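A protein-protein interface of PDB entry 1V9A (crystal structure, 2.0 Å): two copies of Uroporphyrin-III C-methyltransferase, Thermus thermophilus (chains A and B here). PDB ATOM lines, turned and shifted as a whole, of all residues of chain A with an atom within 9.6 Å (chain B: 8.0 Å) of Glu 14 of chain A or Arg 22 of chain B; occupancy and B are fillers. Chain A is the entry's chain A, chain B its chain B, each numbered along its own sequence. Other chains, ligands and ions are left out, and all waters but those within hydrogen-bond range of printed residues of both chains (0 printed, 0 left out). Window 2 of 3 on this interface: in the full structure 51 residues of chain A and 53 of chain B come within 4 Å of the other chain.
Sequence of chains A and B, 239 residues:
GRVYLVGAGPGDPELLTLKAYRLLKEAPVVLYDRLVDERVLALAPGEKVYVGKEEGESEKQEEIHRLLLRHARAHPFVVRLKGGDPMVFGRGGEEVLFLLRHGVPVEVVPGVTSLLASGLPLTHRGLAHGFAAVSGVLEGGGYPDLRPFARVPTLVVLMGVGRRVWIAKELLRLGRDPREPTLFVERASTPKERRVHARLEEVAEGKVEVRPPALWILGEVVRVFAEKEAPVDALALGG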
ATOM      1  N   GLY A   7      11.383 -11.421 -11.126  1.00  0.00           N
ATOM      2  CA  GLY A   7      10.996 -11.100  -9.770  1.00  0.00           C
ATOM      3  C   GLY A   7      10.539  -9.649  -9.736  1.00  0.00           C
ATOM      4  O   GLY A   7      11.272  -8.752 -10.157  1.00  0.00           O
ATOM      5  N   ALA A   8       9.327  -9.407  -9.243  1.00  0.00           N
ATOM      6  CA  ALA A   8       8.802  -8.044  -9.182  1.00  0.00           C
ATOM      7  C   ALA A   8       9.233  -7.286  -7.934  1.00  0.00           C
ATOM      8  O   ALA A   8       8.999  -6.089  -7.830  1.00  0.00           O
ATOM      9  CB  ALA A   8       7.286  -8.065  -9.249  1.00  0.00           C
ATOM     10  N   GLY A   9       9.863  -7.970  -6.990  1.00  0.00           N
ATOM     11  CA  GLY A   9      10.238  -7.292  -5.766  1.00  0.00           C
ATOM     12  C   GLY A   9       9.025  -7.351  -4.840  1.00  0.00           C
ATOM     13  O   GLY A   9       7.944  -7.753  -5.271  1.00  0.00           O
ATOM     14  N   PRO A  10       9.160  -6.939  -3.574  1.00  0.00           N
ATOM     15  CA  PRO A  10       8.053  -6.968  -2.606  1.00  0.00           C
ATOM     16  C   PRO A  10       6.869  -6.007  -2.832  1.00  0.00           C
ATOM     17  O   PRO A  10       5.831  -6.151  -2.181  1.00  0.00           O
ATOM     18  CB  PRO A  10       8.764  -6.720  -1.282  1.00  0.00           C
ATOM     19  CG  PRO A  10       9.842  -5.792  -1.667  1.00  0.00           C
ATOM     20  CD  PRO A  10      10.378  -6.387  -2.958  1.00  0.00           C
ATOM     21  N   GLY A  11       7.002  -5.050  -3.752  1.00  0.00           N
ATOM     22  CA  GLY A  11       5.904  -4.127  -4.004  1.00  0.00           C
ATOM     23  C   GLY A  11       6.317  -2.743  -4.473  1.00  0.00           C
ATOM     24  O   GLY A  11       5.816  -2.247  -5.478  1.00  0.00           O
ATOM     25  N   ASP A  12       7.215  -2.110  -3.730  1.00  0.00           N
ATOM     26  CA  ASP A  12       7.710  -0.790  -4.092  1.00  0.00           C
ATOM     27  C   ASP A  12       8.329  -0.906  -5.490  1.00  0.00           C
ATOM     28  O   ASP A  12       9.266  -1.675  -5.701  1.00  0.00           O
ATOM     29  CB  ASP A  12       8.773  -0.357  -3.093  1.00  0.00           C
ATOM     30  CG  ASP A  12       9.277   1.050  -3.352  1.00  0.00           C
ATOM     31  OD1 ASP A  12       9.080   1.557  -4.473  1.00  0.00           O
ATOM     32  OD2 ASP A  12       9.879   1.647  -2.434  1.00  0.00           O
ATOM     33  N   PRO A  13       7.819  -0.144  -6.465  1.00  0.00           N
ATOM     34  CA  PRO A  13       8.405  -0.258  -7.805  1.00  0.00           C
ATOM     35  C   PRO A  13       9.889   0.064  -7.860  1.00  0.00           C
ATOM     36  O   PRO A  13      10.593  -0.360  -8.783  1.00  0.00           O
ATOM     37  CB  PRO A  13       7.543   0.689  -8.641  1.00  0.00           C
ATOM     38  CG  PRO A  13       7.052   1.689  -7.630  1.00  0.00           C
ATOM     39  CD  PRO A  13       6.719   0.834  -6.448  1.00  0.00           C
ATOM     40  N   GLU A  14      10.374   0.784  -6.857  1.00  0.00           N
ATOM     41  CA  GLU A  14      11.783   1.144  -6.803  1.00  0.00           C
ATOM     42  C   GLU A  14      12.653  -0.046  -6.412  1.00  0.00           C
ATOM     43  O   GLU A  14      13.884   0.028  -6.486  1.00  0.00           O
ATOM     44  CB  GLU A  14      12.010   2.279  -5.805  1.00  0.00           C
ATOM     45  CG  GLU A  14      11.414   3.609  -6.238  1.00  0.00           C
ATOM     46  CD  GLU A  14      12.206   4.273  -7.348  1.00  0.00           C
ATOM     47  OE1 GLU A  14      13.302   4.810  -7.062  1.00  0.00           O
ATOM     48  OE2 GLU A  14      11.732   4.253  -8.507  1.00  0.00           O
ATOM     49  N   LEU A  15      12.027  -1.136  -5.978  1.00  0.00           N
ATOM     50  CA  LEU A  15      12.806  -2.303  -5.599  1.00  0.00           C
ATOM     51  C   LEU A  15      12.855  -3.338  -6.723  1.00  0.00           C
ATOM     52  O   LEU A  15      13.275  -4.473  -6.524  1.00  0.00           O
ATOM     53  CB  LEU A  15      12.289  -2.909  -4.299  1.00  0.00           C
ATOM     54  CG  LEU A  15      12.496  -1.962  -3.106  1.00  0.00           C
ATOM     55  CD1 LEU A  15      12.045  -2.624  -1.808  1.00  0.00           C
ATOM     56  CD2 LEU A  15      13.954  -1.570  -3.017  1.00  0.00           C
ATOM     57  N   LEU A  16      12.396  -2.933  -7.900  1.00  0.00           N
ATOM     58  CA  LEU A  16      12.474  -3.775  -9.072  1.00  0.00           C
ATOM     59  C   LEU A  16      13.973  -3.698  -9.398  1.00  0.00           C
ATOM     60  O   LEU A  16      14.633  -2.734  -9.009  1.00  0.00           O
ATOM     61  CB  LEU A  16      11.716  -3.150 -10.239  1.00  0.00           C
ATOM     62  CG  LEU A  16      10.233  -3.452 -10.448  1.00  0.00           C
ATOM     63  CD1 LEU A  16       9.700  -2.566 -11.551  1.00  0.00           C
ATOM     64  CD2 LEU A  16      10.053  -4.930 -10.825  1.00  0.00           C
ATOM     65  N   THR A  17      14.514  -4.700 -10.083  1.00  0.00           N
ATOM     66  CA  THR A  17      15.913  -4.635 -10.493  1.00  0.00           C
ATOM     67  C   THR A  17      15.904  -3.839 -11.790  1.00  0.00           C
ATOM     68  O   THR A  17      14.859  -3.704 -12.429  1.00  0.00           O
ATOM     69  CB  THR A  17      16.513  -6.033 -10.826  1.00  0.00           C
ATOM     70  OG1 THR A  17      15.687  -6.697 -11.791  1.00  0.00           O
ATOM     71  CG2 THR A  17      16.638  -6.868  -9.575  1.00  0.00           C
ATOM     72  N   LEU A  18      17.059  -3.337 -12.206  1.00  0.00           N
ATOM     73  CA  LEU A  18      17.121  -2.610 -13.479  1.00  0.00           C
ATOM     74  C   LEU A  18      16.696  -3.538 -14.620  1.00  0.00           C
ATOM     75  O   LEU A  18      15.999  -3.129 -15.546  1.00  0.00           O
ATOM     76  CB  LEU A  18      18.542  -2.118 -13.750  1.00  0.00           C
ATOM     77  CG  LEU A  18      19.069  -1.162 -12.679  1.00  0.00           C
ATOM     78  CD1 LEU A  18      20.491  -0.765 -13.010  1.00  0.00           C
ATOM     79  CD2 LEU A  18      18.171   0.055 -12.598  1.00  0.00           C
ATOM     80  N   ALA A  20      14.663  -6.219 -14.492  1.00  0.00           N
ATOM     81  CA  ALA A  20      13.219  -6.440 -14.436  1.00  0.00           C
ATOM     82  C   ALA A  20      12.494  -5.246 -15.048  1.00  0.00           C
ATOM     83  O   ALA A  20      11.542  -5.400 -15.825  1.00  0.00           O
ATOM     84  CB  ALA A  20      12.761  -6.630 -12.965  1.00  0.00           C
ATOM     85  N   TYR A  21      12.952  -4.051 -14.690  1.00  0.00           N
ATOM     86  CA  TYR A  21      12.344  -2.821 -15.187  1.00  0.00           C
ATOM     87  C   TYR A  21      12.441  -2.744 -16.697  1.00  0.00           C
ATOM     88  O   TYR A  21      11.462  -2.432 -17.373  1.00  0.00           O
ATOM     89  CB  TYR A  21      13.027  -1.609 -14.566  1.00  0.00           C
ATOM     90  CG  TYR A  21      12.473  -0.288 -15.052  1.00  0.00           C
ATOM     91  CD1 TYR A  21      11.235   0.183 -14.614  1.00  0.00           C
ATOM     92  CD2 TYR A  21      13.183   0.479 -15.971  1.00  0.00           C
ATOM     93  CE1 TYR A  21      10.717   1.398 -15.089  1.00  0.00           C
ATOM     94  CE2 TYR A  21      12.682   1.678 -16.448  1.00  0.00           C
ATOM     95  CZ  TYR A  21      11.452   2.132 -16.008  1.00  0.00           C
ATOM     96  OH  TYR A  21      10.970   3.314 -16.512  1.00  0.00           O
ATOM     97  N   LYS A  25       9.115  -2.818 -19.265  1.00  0.00           N
ATOM     98  CA  LYS A  25       8.845  -1.680 -20.141  1.00  0.00           C
ATOM     99  C   LYS A  25       8.784  -2.082 -21.612  1.00  0.00           C
ATOM    100  O   LYS A  25       8.154  -1.396 -22.409  1.00  0.00           O
ATOM    101  CB  LYS A  25       9.928  -0.607 -19.995  1.00  0.00           C
ATOM    102  CG  LYS A  25       9.975   0.109 -18.646  1.00  0.00           C
ATOM    103  CD  LYS A  25       8.626   0.723 -18.270  1.00  0.00           C
ATOM    104  CE  LYS A  25       8.201   1.818 -19.235  1.00  0.00           C
ATOM    105  NZ  LYS A  25       6.878   2.377 -18.828  1.00  0.00           N
ATOM    106  N   ASP A  37       2.589  -6.141  -7.021  1.00  0.00           N
ATOM    107  CA  ASP A  37       2.057  -4.798  -6.744  1.00  0.00           C
ATOM    108  C   ASP A  37       1.471  -4.078  -7.959  1.00  0.00           C
ATOM    109  O   ASP A  37       2.028  -4.107  -9.057  1.00  0.00           O
ATOM    110  CB  ASP A  37       3.138  -3.938  -6.089  1.00  0.00           C
ATOM    111  CG  ASP A  37       2.566  -2.747  -5.339  1.00  0.00           C
ATOM    112  OD1 ASP A  37       2.034  -1.831  -5.994  1.00  0.00           O
ATOM    113  OD2 ASP A  37       2.664  -2.728  -4.094  1.00  0.00           O
ATOM    114  N   ARG A  39       1.439  -1.055  -8.638  1.00  0.00           N
ATOM    115  CA  ARG A  39       2.329  -0.014  -9.144  1.00  0.00           C
ATOM    116  C   ARG A  39       3.407  -0.575 -10.062  1.00  0.00           C
ATOM    117  O   ARG A  39       3.956   0.141 -10.900  1.00  0.00           O
ATOM    118  CB  ARG A  39       3.004   0.714  -7.989  1.00  0.00           C
ATOM    119  CG  ARG A  39       2.078   1.602  -7.174  1.00  0.00           C
ATOM    120  CD  ARG A  39       2.764   1.972  -5.872  1.00  0.00           C
ATOM    121  NE  ARG A  39       2.971   0.777  -5.057  1.00  0.00           N
ATOM    122  CZ  ARG A  39       3.779   0.712  -4.005  1.00  0.00           C
ATOM    123  NH1 ARG A  39       4.473   1.777  -3.624  1.00  0.00           N
ATOM    124  NH2 ARG A  39       3.889  -0.423  -3.330  1.00  0.00           N
ATOM    125  N   VAL A  40       3.732  -1.848  -9.876  1.00  0.00           N
ATOM    126  CA  VAL A  40       4.728  -2.491 -10.716  1.00  0.00           C
ATOM    127  C   VAL A  40       4.083  -2.735 -12.081  1.00  0.00           C
ATOM    128  O   VAL A  40       4.653  -2.393 -13.118  1.00  0.00           O
ATOM    129  CB  VAL A  40       5.208  -3.816 -10.091  1.00  0.00           C
ATOM    130  CG1 VAL A  40       5.831  -4.719 -11.160  1.00  0.00           C
ATOM    131  CG2 VAL A  40       6.231  -3.519  -8.997  1.00  0.00           C
ATOM    132  N   LEU A  43       3.587  -0.031 -14.796  1.00  0.00           N
ATOM    133  CA  LEU A  43       4.800   0.329 -15.528  1.00  0.00           C
ATOM    134  C   LEU A  43       4.910  -0.390 -16.861  1.00  0.00           C
ATOM    135  O   LEU A  43       5.627   0.054 -17.750  1.00  0.00           O
ATOM    136  CB  LEU A  43       6.045  -0.024 -14.717  1.00  0.00           C
ATOM    137  CG  LEU A  43       6.305   0.758 -13.441  1.00  0.00           C
ATOM    138  CD1 LEU A  43       7.626   0.316 -12.813  1.00  0.00           C
ATOM    139  CD2 LEU A  43       6.346   2.233 -13.786  1.00  0.00           C
ATOM    140  N   VAL A 112      14.162  -8.816  -5.317  1.00  0.00           N
ATOM    141  CA  VAL A 112      14.227  -8.610  -3.885  1.00  0.00           C
ATOM    142  C   VAL A 112      13.076  -9.442  -3.324  1.00  0.00           C
ATOM    143  O   VAL A 112      11.917  -9.141  -3.571  1.00  0.00           O
ATOM    144  CB  VAL A 112      14.008  -7.122  -3.523  1.00  0.00           C
ATOM    145  CG1 VAL A 112      13.875  -6.963  -2.008  1.00  0.00           C
ATOM    146  CG2 VAL A 112      15.160  -6.290  -4.057  1.00  0.00           C
ATOM    147  N   SER A 189       7.117  -2.844   2.353  1.00  0.00           N
ATOM    148  CA  SER A 189       7.530  -1.964   1.270  1.00  0.00           C
ATOM    149  C   SER A 189       6.375  -1.273   0.551  1.00  0.00           C
ATOM    150  O   SER A 189       6.539  -0.773  -0.563  1.00  0.00           O
ATOM    151  CB  SER A 189       8.392  -2.737   0.266  1.00  0.00           C
ATOM    152  OG  SER A 189       7.644  -3.081  -0.870  1.00  0.00           O
ATOM    153  N   LEU B  16      20.912  -4.447  -9.775  1.00  0.00           N
ATOM    154  CA  LEU B  16      20.836  -3.383  -8.777  1.00  0.00           C
ATOM    155  C   LEU B  16      19.343  -3.025  -8.763  1.00  0.00           C
ATOM    156  O   LEU B  16      18.669  -3.187  -9.790  1.00  0.00           O
ATOM    157  CB  LEU B  16      21.607  -2.149  -9.269  1.00  0.00           C
ATOM    158  CG  LEU B  16      23.114  -2.066  -9.083  1.00  0.00           C
ATOM    159  CD1 LEU B  16      23.705  -0.917  -9.927  1.00  0.00           C
ATOM    160  CD2 LEU B  16      23.402  -1.867  -7.606  1.00  0.00           C
ATOM    161  N   THR B  17      18.815  -2.561  -7.634  1.00  0.00           N
ATOM    162  CA  THR B  17      17.417  -2.136  -7.607  1.00  0.00           C
ATOM    163  C   THR B  17      17.414  -0.741  -8.226  1.00  0.00           C
ATOM    164  O   THR B  17      18.460  -0.097  -8.301  1.00  0.00           O
ATOM    165  CB  THR B  17      16.853  -2.009  -6.173  1.00  0.00           C
ATOM    166  OG1 THR B  17      17.719  -1.179  -5.380  1.00  0.00           O
ATOM    167  CG2 THR B  17      16.705  -3.379  -5.525  1.00  0.00           C
ATOM    168  N   LEU B  18      16.255  -0.280  -8.686  1.00  0.00           N
ATOM    169  CA  LEU B  18      16.163   1.071  -9.267  1.00  0.00           C
ATOM    170  C   LEU B  18      16.576   2.096  -8.230  1.00  0.00           C
ATOM    171  O   LEU B  18      17.311   3.031  -8.541  1.00  0.00           O
ATOM    172  CB  LEU B  18      14.747   1.400  -9.687  1.00  0.00           C
ATOM    173  CG  LEU B  18      14.216   0.496 -10.791  1.00  0.00           C
ATOM    174  CD1 LEU B  18      12.835   0.966 -11.211  1.00  0.00           C
ATOM    175  CD2 LEU B  18      15.159   0.559 -11.959  1.00  0.00           C
ATOM    176  N   LYS B  19      16.090   1.925  -7.000  1.00  0.00           N
ATOM    177  CA  LYS B  19      16.431   2.834  -5.905  1.00  0.00           C
ATOM    178  C   LYS B  19      17.943   2.899  -5.679  1.00  0.00           C
ATOM    179  O   LYS B  19      18.502   3.975  -5.483  1.00  0.00           O
ATOM    180  CB  LYS B  19      15.743   2.388  -4.611  1.00  0.00           C
ATOM    181  CG  LYS B  19      15.715   3.452  -3.508  1.00  0.00           C
ATOM    182  CD  LYS B  19      14.766   3.038  -2.393  1.00  0.00           C
ATOM    183  CE  LYS B  19      14.786   4.055  -1.280  1.00  0.00           C
ATOM    184  NZ  LYS B  19      14.140   3.522  -0.058  1.00  0.00           N
ATOM    185  N   ALA B  20      18.605   1.743  -5.713  1.00  0.00           N
ATOM    186  CA  ALA B  20      20.057   1.689  -5.504  1.00  0.00           C
ATOM    187  C   ALA B  20      20.802   2.396  -6.638  1.00  0.00           C
ATOM    188  O   ALA B  20      21.786   3.102  -6.406  1.00  0.00           O
ATOM    189  CB  ALA B  20      20.538   0.225  -5.396  1.00  0.00           C
ATOM    190  N   TYR B  21      20.325   2.204  -7.862  1.00  0.00           N
ATOM    191  CA  TYR B  21      20.936   2.819  -9.031  1.00  0.00           C
ATOM    192  C   TYR B  21      20.833   4.348  -8.909  1.00  0.00           C
ATOM    193  O   TYR B  21      21.815   5.070  -9.045  1.00  0.00           O
ATOM    194  CB  TYR B  21      20.201   2.353 -10.283  1.00  0.00           C
ATOM    195  CG  TYR B  21      20.604   3.082 -11.541  1.00  0.00           C
ATOM    196  CD1 TYR B  21      21.807   2.795 -12.184  1.00  0.00           C
ATOM    197  CD2 TYR B  21      19.772   4.061 -12.095  1.00  0.00           C
ATOM    198  CE1 TYR B  21      22.176   3.459 -13.351  1.00  0.00           C
ATOM    199  CE2 TYR B  21      20.132   4.734 -13.263  1.00  0.00           C
ATOM    200  CZ  TYR B  21      21.330   4.427 -13.884  1.00  0.00           C
ATOM    201  OH  TYR B  21      21.668   5.064 -15.046  1.00  0.00           O
ATOM    202  N   ARG B  22      19.630   4.835  -8.657  1.00  0.00           N
ATOM    203  CA  ARG B  22      19.417   6.265  -8.518  1.00  0.00           C
ATOM    204  C   ARG B  22      20.263   6.847  -7.389  1.00  0.00           C
ATOM    205  O   ARG B  22      20.862   7.914  -7.556  1.00  0.00           O
ATOM    206  CB  ARG B  22      17.935   6.534  -8.295  1.00  0.00           C
ATOM    207  CG  ARG B  22      17.121   6.131  -9.518  1.00  0.00           C
ATOM    208  CD  ARG B  22      15.615   6.200  -9.306  1.00  0.00           C
ATOM    209  NE  ARG B  22      14.926   5.752 -10.515  1.00  0.00           N
ATOM    210  CZ  ARG B  22      13.610   5.748 -10.680  1.00  0.00           C
ATOM    211  NH1 ARG B  22      12.815   6.173  -9.707  1.00  0.00           N
ATOM    212  NH2 ARG B  22      13.087   5.318 -11.822  1.00  0.00           N
ATOM    213  N   LEU B  23      20.323   6.154  -6.253  1.00  0.00           N
ATOM    214  CA  LEU B  23      21.132   6.639  -5.139  1.00  0.00           C
ATOM    215  C   LEU B  23      22.605   6.672  -5.513  1.00  0.00           C
ATOM    216  O   LEU B  23      23.318   7.606  -5.134  1.00  0.00           O
ATOM    217  CB  LEU B  23      20.937   5.777  -3.896  1.00  0.00           C
ATOM    218  CG  LEU B  23      19.632   5.979  -3.120  1.00  0.00           C
ATOM    219  CD1 LEU B  23      19.474   4.876  -2.082  1.00  0.00           C
ATOM    220  CD2 LEU B  23      19.645   7.357  -2.442  1.00  0.00           C
ATOM    221  N   LEU B  24      23.069   5.673  -6.268  1.00  0.00           N
ATOM    222  CA  LEU B  24      24.485   5.634  -6.658  1.00  0.00           C
ATOM    223  C   LEU B  24      24.852   6.763  -7.603  1.00  0.00           C
ATOM    224  O   LEU B  24      25.932   7.339  -7.499  1.00  0.00           O
ATOM    225  CB  LEU B  24      24.848   4.301  -7.329  1.00  0.00           C
ATOM    226  CG  LEU B  24      24.899   3.068  -6.425  1.00  0.00           C
ATOM    227  CD1 LEU B  24      25.220   1.842  -7.282  1.00  0.00           C
ATOM    228  CD2 LEU B  24      25.958   3.262  -5.334  1.00  0.00           C
ATOM    229  N   LYS B  25      23.956   7.050  -8.543  1.00  0.00           N
ATOM    230  CA  LYS B  25      24.178   8.118  -9.505  1.00  0.00           C
ATOM    231  C   LYS B  25      24.191   9.466  -8.784  1.00  0.00           C
ATOM    232  O   LYS B  25      24.980  10.361  -9.117  1.00  0.00           O
ATOM    233  CB  LYS B  25      23.057   8.133 -10.555  1.00  0.00           C
ATOM    234  CG  LYS B  25      22.905   6.832 -11.347  1.00  0.00           C
ATOM    235  CD  LYS B  25      24.142   6.495 -12.168  1.00  0.00           C
ATOM    236  CE  LYS B  25      24.337   7.433 -13.344  1.00  0.00           C
ATOM    237  NZ  LYS B  25      25.561   7.048 -14.108  1.00  0.00           N
ATOM    238  N   GLU B  26      23.325   9.589  -7.782  1.00  0.00           N
ATOM    239  CA  GLU B  26      23.162  10.840  -7.042  1.00  0.00           C
ATOM    240  C   GLU B  26      24.026  11.094  -5.809  1.00  0.00           C
ATOM    241  O   GLU B  26      24.239  12.254  -5.428  1.00  0.00           O
ATOM    242  CB  GLU B  26      21.692  10.994  -6.647  1.00  0.00           C
ATOM    243  CG  GLU B  26      20.776  11.141  -7.865  1.00  0.00           C
ATOM    244  CD  GLU B  26      19.300  11.060  -7.534  1.00  0.00           C
ATOM    245  OE1 GLU B  26      18.940  11.177  -6.340  1.00  0.00           O
ATOM    246  OE2 GLU B  26      18.503  10.890  -8.484  1.00  0.00           O
ATOM    247  N   ALA B  27      24.541  10.033  -5.199  1.00  0.00           N
ATOM    248  CA  ALA B  27      25.333  10.155  -3.974  1.00  0.00           C
ATOM    249  C   ALA B  27      26.655  10.904  -4.066  1.00  0.00           C
ATOM    250  O   ALA B  27      27.478  10.640  -4.948  1.00  0.00           O
ATOM    251  CB  ALA B  27      25.576   8.771  -3.387  1.00  0.00           C
ATOM    252  N   LEU B  43      29.343   3.052 -11.971  1.00  0.00           N
ATOM    253  CA  LEU B  43      28.098   3.760 -12.250  1.00  0.00           C
ATOM    254  C   LEU B  43      28.003   4.979 -11.330  1.00  0.00           C
ATOM    255  O   LEU B  43      27.272   5.930 -11.609  1.00  0.00           O
ATOM    256  CB  LEU B  43      26.896   2.839 -12.020  1.00  0.00           C
ATOM    257  CG  LEU B  43      26.725   1.665 -12.995  1.00  0.00           C
ATOM    258  CD1 LEU B  43      25.488   0.871 -12.609  1.00  0.00           C
ATOM    259  CD2 LEU B  43      26.592   2.173 -14.428  1.00  0.00           C
ATOM    260  N   PRO B  45      29.323   8.361  -9.787  1.00  0.00           N
ATOM    261  CA  PRO B  45      30.250   9.436 -10.165  1.00  0.00           C
ATOM    262  C   PRO B  45      30.805  10.213  -8.973  1.00  0.00           C
ATOM    263  O   PRO B  45      31.745  10.991  -9.119  1.00  0.00           O
ATOM    264  CB  PRO B  45      29.398  10.305 -11.082  1.00  0.00           C
ATOM    265  CG  PRO B  45      28.047  10.231 -10.428  1.00  0.00           C
ATOM    266  CD  PRO B  45      27.921   8.757 -10.038  1.00  0.00           C
ATOM    267  N   PHE B  77      23.629  13.315   2.729  1.00  0.00           N
ATOM    268  CA  PHE B  77      23.401  11.878   2.769  1.00  0.00           C
ATOM    269  C   PHE B  77      24.563  11.175   2.098  1.00  0.00           C
ATOM    270  O   PHE B  77      25.281  11.759   1.276  1.00  0.00           O
ATOM    271  CB  PHE B  77      22.083  11.511   2.068  1.00  0.00           C
ATOM    272  CG  PHE B  77      22.165  11.470   0.561  1.00  0.00           C
ATOM    273  CD1 PHE B  77      22.647  10.338  -0.098  1.00  0.00           C
ATOM    274  CD2 PHE B  77      21.730  12.550  -0.201  1.00  0.00           C
ATOM    275  CE1 PHE B  77      22.688  10.284  -1.493  1.00  0.00           C
ATOM    276  CE2 PHE B  77      21.767  12.507  -1.599  1.00  0.00           C
ATOM    277  CZ  PHE B  77      22.246  11.369  -2.246  1.00  0.00           C
ATOM    278  N   VAL B  79      25.928   6.983   0.771  1.00  0.00           N
ATOM    279  CA  VAL B  79      25.496   5.632   0.464  1.00  0.00           C
ATOM    280  C   VAL B  79      26.562   4.682   0.961  1.00  0.00           C
ATOM    281  O   VAL B  79      27.745   4.837   0.632  1.00  0.00           O
ATOM    282  CB  VAL B  79      25.334   5.407  -1.058  1.00  0.00           C
ATOM    283  CG1 VAL B  79      25.237   3.908  -1.363  1.00  0.00           C
ATOM    284  CG2 VAL B  79      24.083   6.118  -1.556  1.00  0.00           C
ATOM    285  N   VAL B 109      18.106  -0.261   2.047  1.00  0.00           N
ATOM    286  CA  VAL B 109      17.591  -0.499   0.704  1.00  0.00           C
ATOM    287  C   VAL B 109      17.964  -1.940   0.368  1.00  0.00           C
ATOM    288  O   VAL B 109      19.124  -2.242   0.075  1.00  0.00           O
ATOM    289  CB  VAL B 109      18.229   0.439  -0.333  1.00  0.00           C
ATOM    290  CG1 VAL B 109      17.606   0.171  -1.717  1.00  0.00           C
ATOM    291  CG2 VAL B 109      18.012   1.910   0.075  1.00  0.00           C
ATOM    292  N   PRO B 110      16.988  -2.853   0.442  1.00  0.00           N
ATOM    293  CA  PRO B 110      17.194  -4.277   0.150  1.00  0.00           C
ATOM    294  C   PRO B 110      17.771  -4.493  -1.241  1.00  0.00           C
ATOM    295  O   PRO B 110      17.686  -3.620  -2.110  1.00  0.00           O
ATOM    296  CB  PRO B 110      15.790  -4.869   0.273  1.00  0.00           C
ATOM    297  CG  PRO B 110      15.112  -3.954   1.240  1.00  0.00           C
ATOM    298  CD  PRO B 110      15.581  -2.592   0.782  1.00  0.00           C
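Glu 14 of chain A touches just these residues of chain B: Thr 17 (3.6 Å), Leu 18 (3.2 Å), Lys 19 (3.0 Å) and Arg 22 (2.5 Å).
Arg 22 of chain B touches just one residue of chain A: Glu 14.
Leu 18 of chain B touches just these residues of chain A: Pro 13, Glu 14, Leu 16, Leu 18 and Tyr 21.
Of the printed residues of chain A, Leu 16 of chain B touches Thr 17 and Leu 18.
Printed residues of chain A within 4 Å of Tyr 21 of chain B: Leu 18.
Of the printed residues of chain A, Lys 19 of chain B touches Glu 14.
Printed residues of chain B within 4 Å of Tyr 21 of chain A: Leu 18 (3.8 Å).
Printed residues of chain A within 4 Å of Thr 17 of chain B: Glu 14, Leu 15, Leu 16 and Val 112.
Pro 45 of chain B touches none of the printed residues of chain A.
The nearest residue of chain B that does not touch Glu 14 of chain A is Ala 20 of chain B (5.1 Å).
Leu 16 of chain A touches Thr 17 of chain B, and with the chains exchanged Thr 17 of chain A touches Leu 16 of chain B.
Leu 16 of chain A touches Leu 18 of chain B, and with the chains exchanged Leu 18 of chain A touches Leu 16 of chain B.
Leu 18 of chain B touches its own counterpart, Leu 18 of chain A.
7 positions are printed for both chains.
The backbone NH (N) of Glu 14 of chain A lies within hydrogen-bond range of the side-chain carboxylate (OD1) of Asp 12 of chain A (2.8 Å).
The side-chain hydroxyl (OG1) of Thr 17 of chain A is in hydrogen-bond range of the backbone NH (N) of Ala 20 of chain A (2.9 Å).
OG1 of Thr 17 of chain B sits at hydrogen-bond distance from N of Ala 20 of chain B.
Among the printed residues, pairs that only touch across the chains: Leu 18 of chain A with Leu 18 of chain B (3.1 Å), Leu 16 of chain A with Thr 17 of chain B (3.2 Å), Thr 17 of chain A with Leu 16 of chain B (3.2 Å), Pro 13 of chain A with Leu 18 of chain B (3.6 Å), Val 112 of chain A with Thr 17 of chain B (3.6 Å), Glu 14 of chain A with Thr 17 of chain B (3.6 Å), Val 112 of chain A with Pro 110 of chain B (3.6 Å), Leu 15 of chain A with Thr 17 of chain B (3.7 Å), Tyr 21 of chain A with Leu 18 of chain B (3.8 Å) and Leu 18 of chain A with Tyr 21 of chain B (3.8 Å).
Of the 18 printed residues of chain B, 7 touch a printed residue of chain A.
Printed residues of chain B that touch a printed residue of chain A: Leu 16, Thr 17, Leu 18, Lys 19, Tyr 21, Arg 22 and Pro 110.
Hydrophobic or aromatic side chains of chain B within 4 Å of the printed part of chain A: Leu 18, Tyr 21 and Pro 110.
Of the 21 printed residues of chain A, 8 touch a printed residue of chain B.
Hydrophobic or aromatic side chains of chain A that line the printed part of chain B: Leu 18, Tyr 21 and Val 112.
Among the printed residues, 15 pairs touch across the chains.
The backbone carbonyl oxygen (O) of Glu 14 of chain A lies within hydrogen-bond range of the backbone NH (N) of Leu 18 of chain B, at 3.2 Å.
N of Lys 19 of chain B sits at hydrogen-bond distance from O of Glu 14 of chain A, 3.0 Å away.
The guanidinium group of Arg 22 of chain B is in salt-bridge range of the side-chain carboxylate of Glu 14 of chain A, at 2.5 Å.
N of Leu 18 of chain B lies within hydrogen-bond range of O of Leu 16 of chain A, 3.0 Å away.
The backbone NH of Leu 18 of chain A lies within hydrogen-bond range of the backbone carbonyl oxygen of Leu 16 of chain B (2.9 Å).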
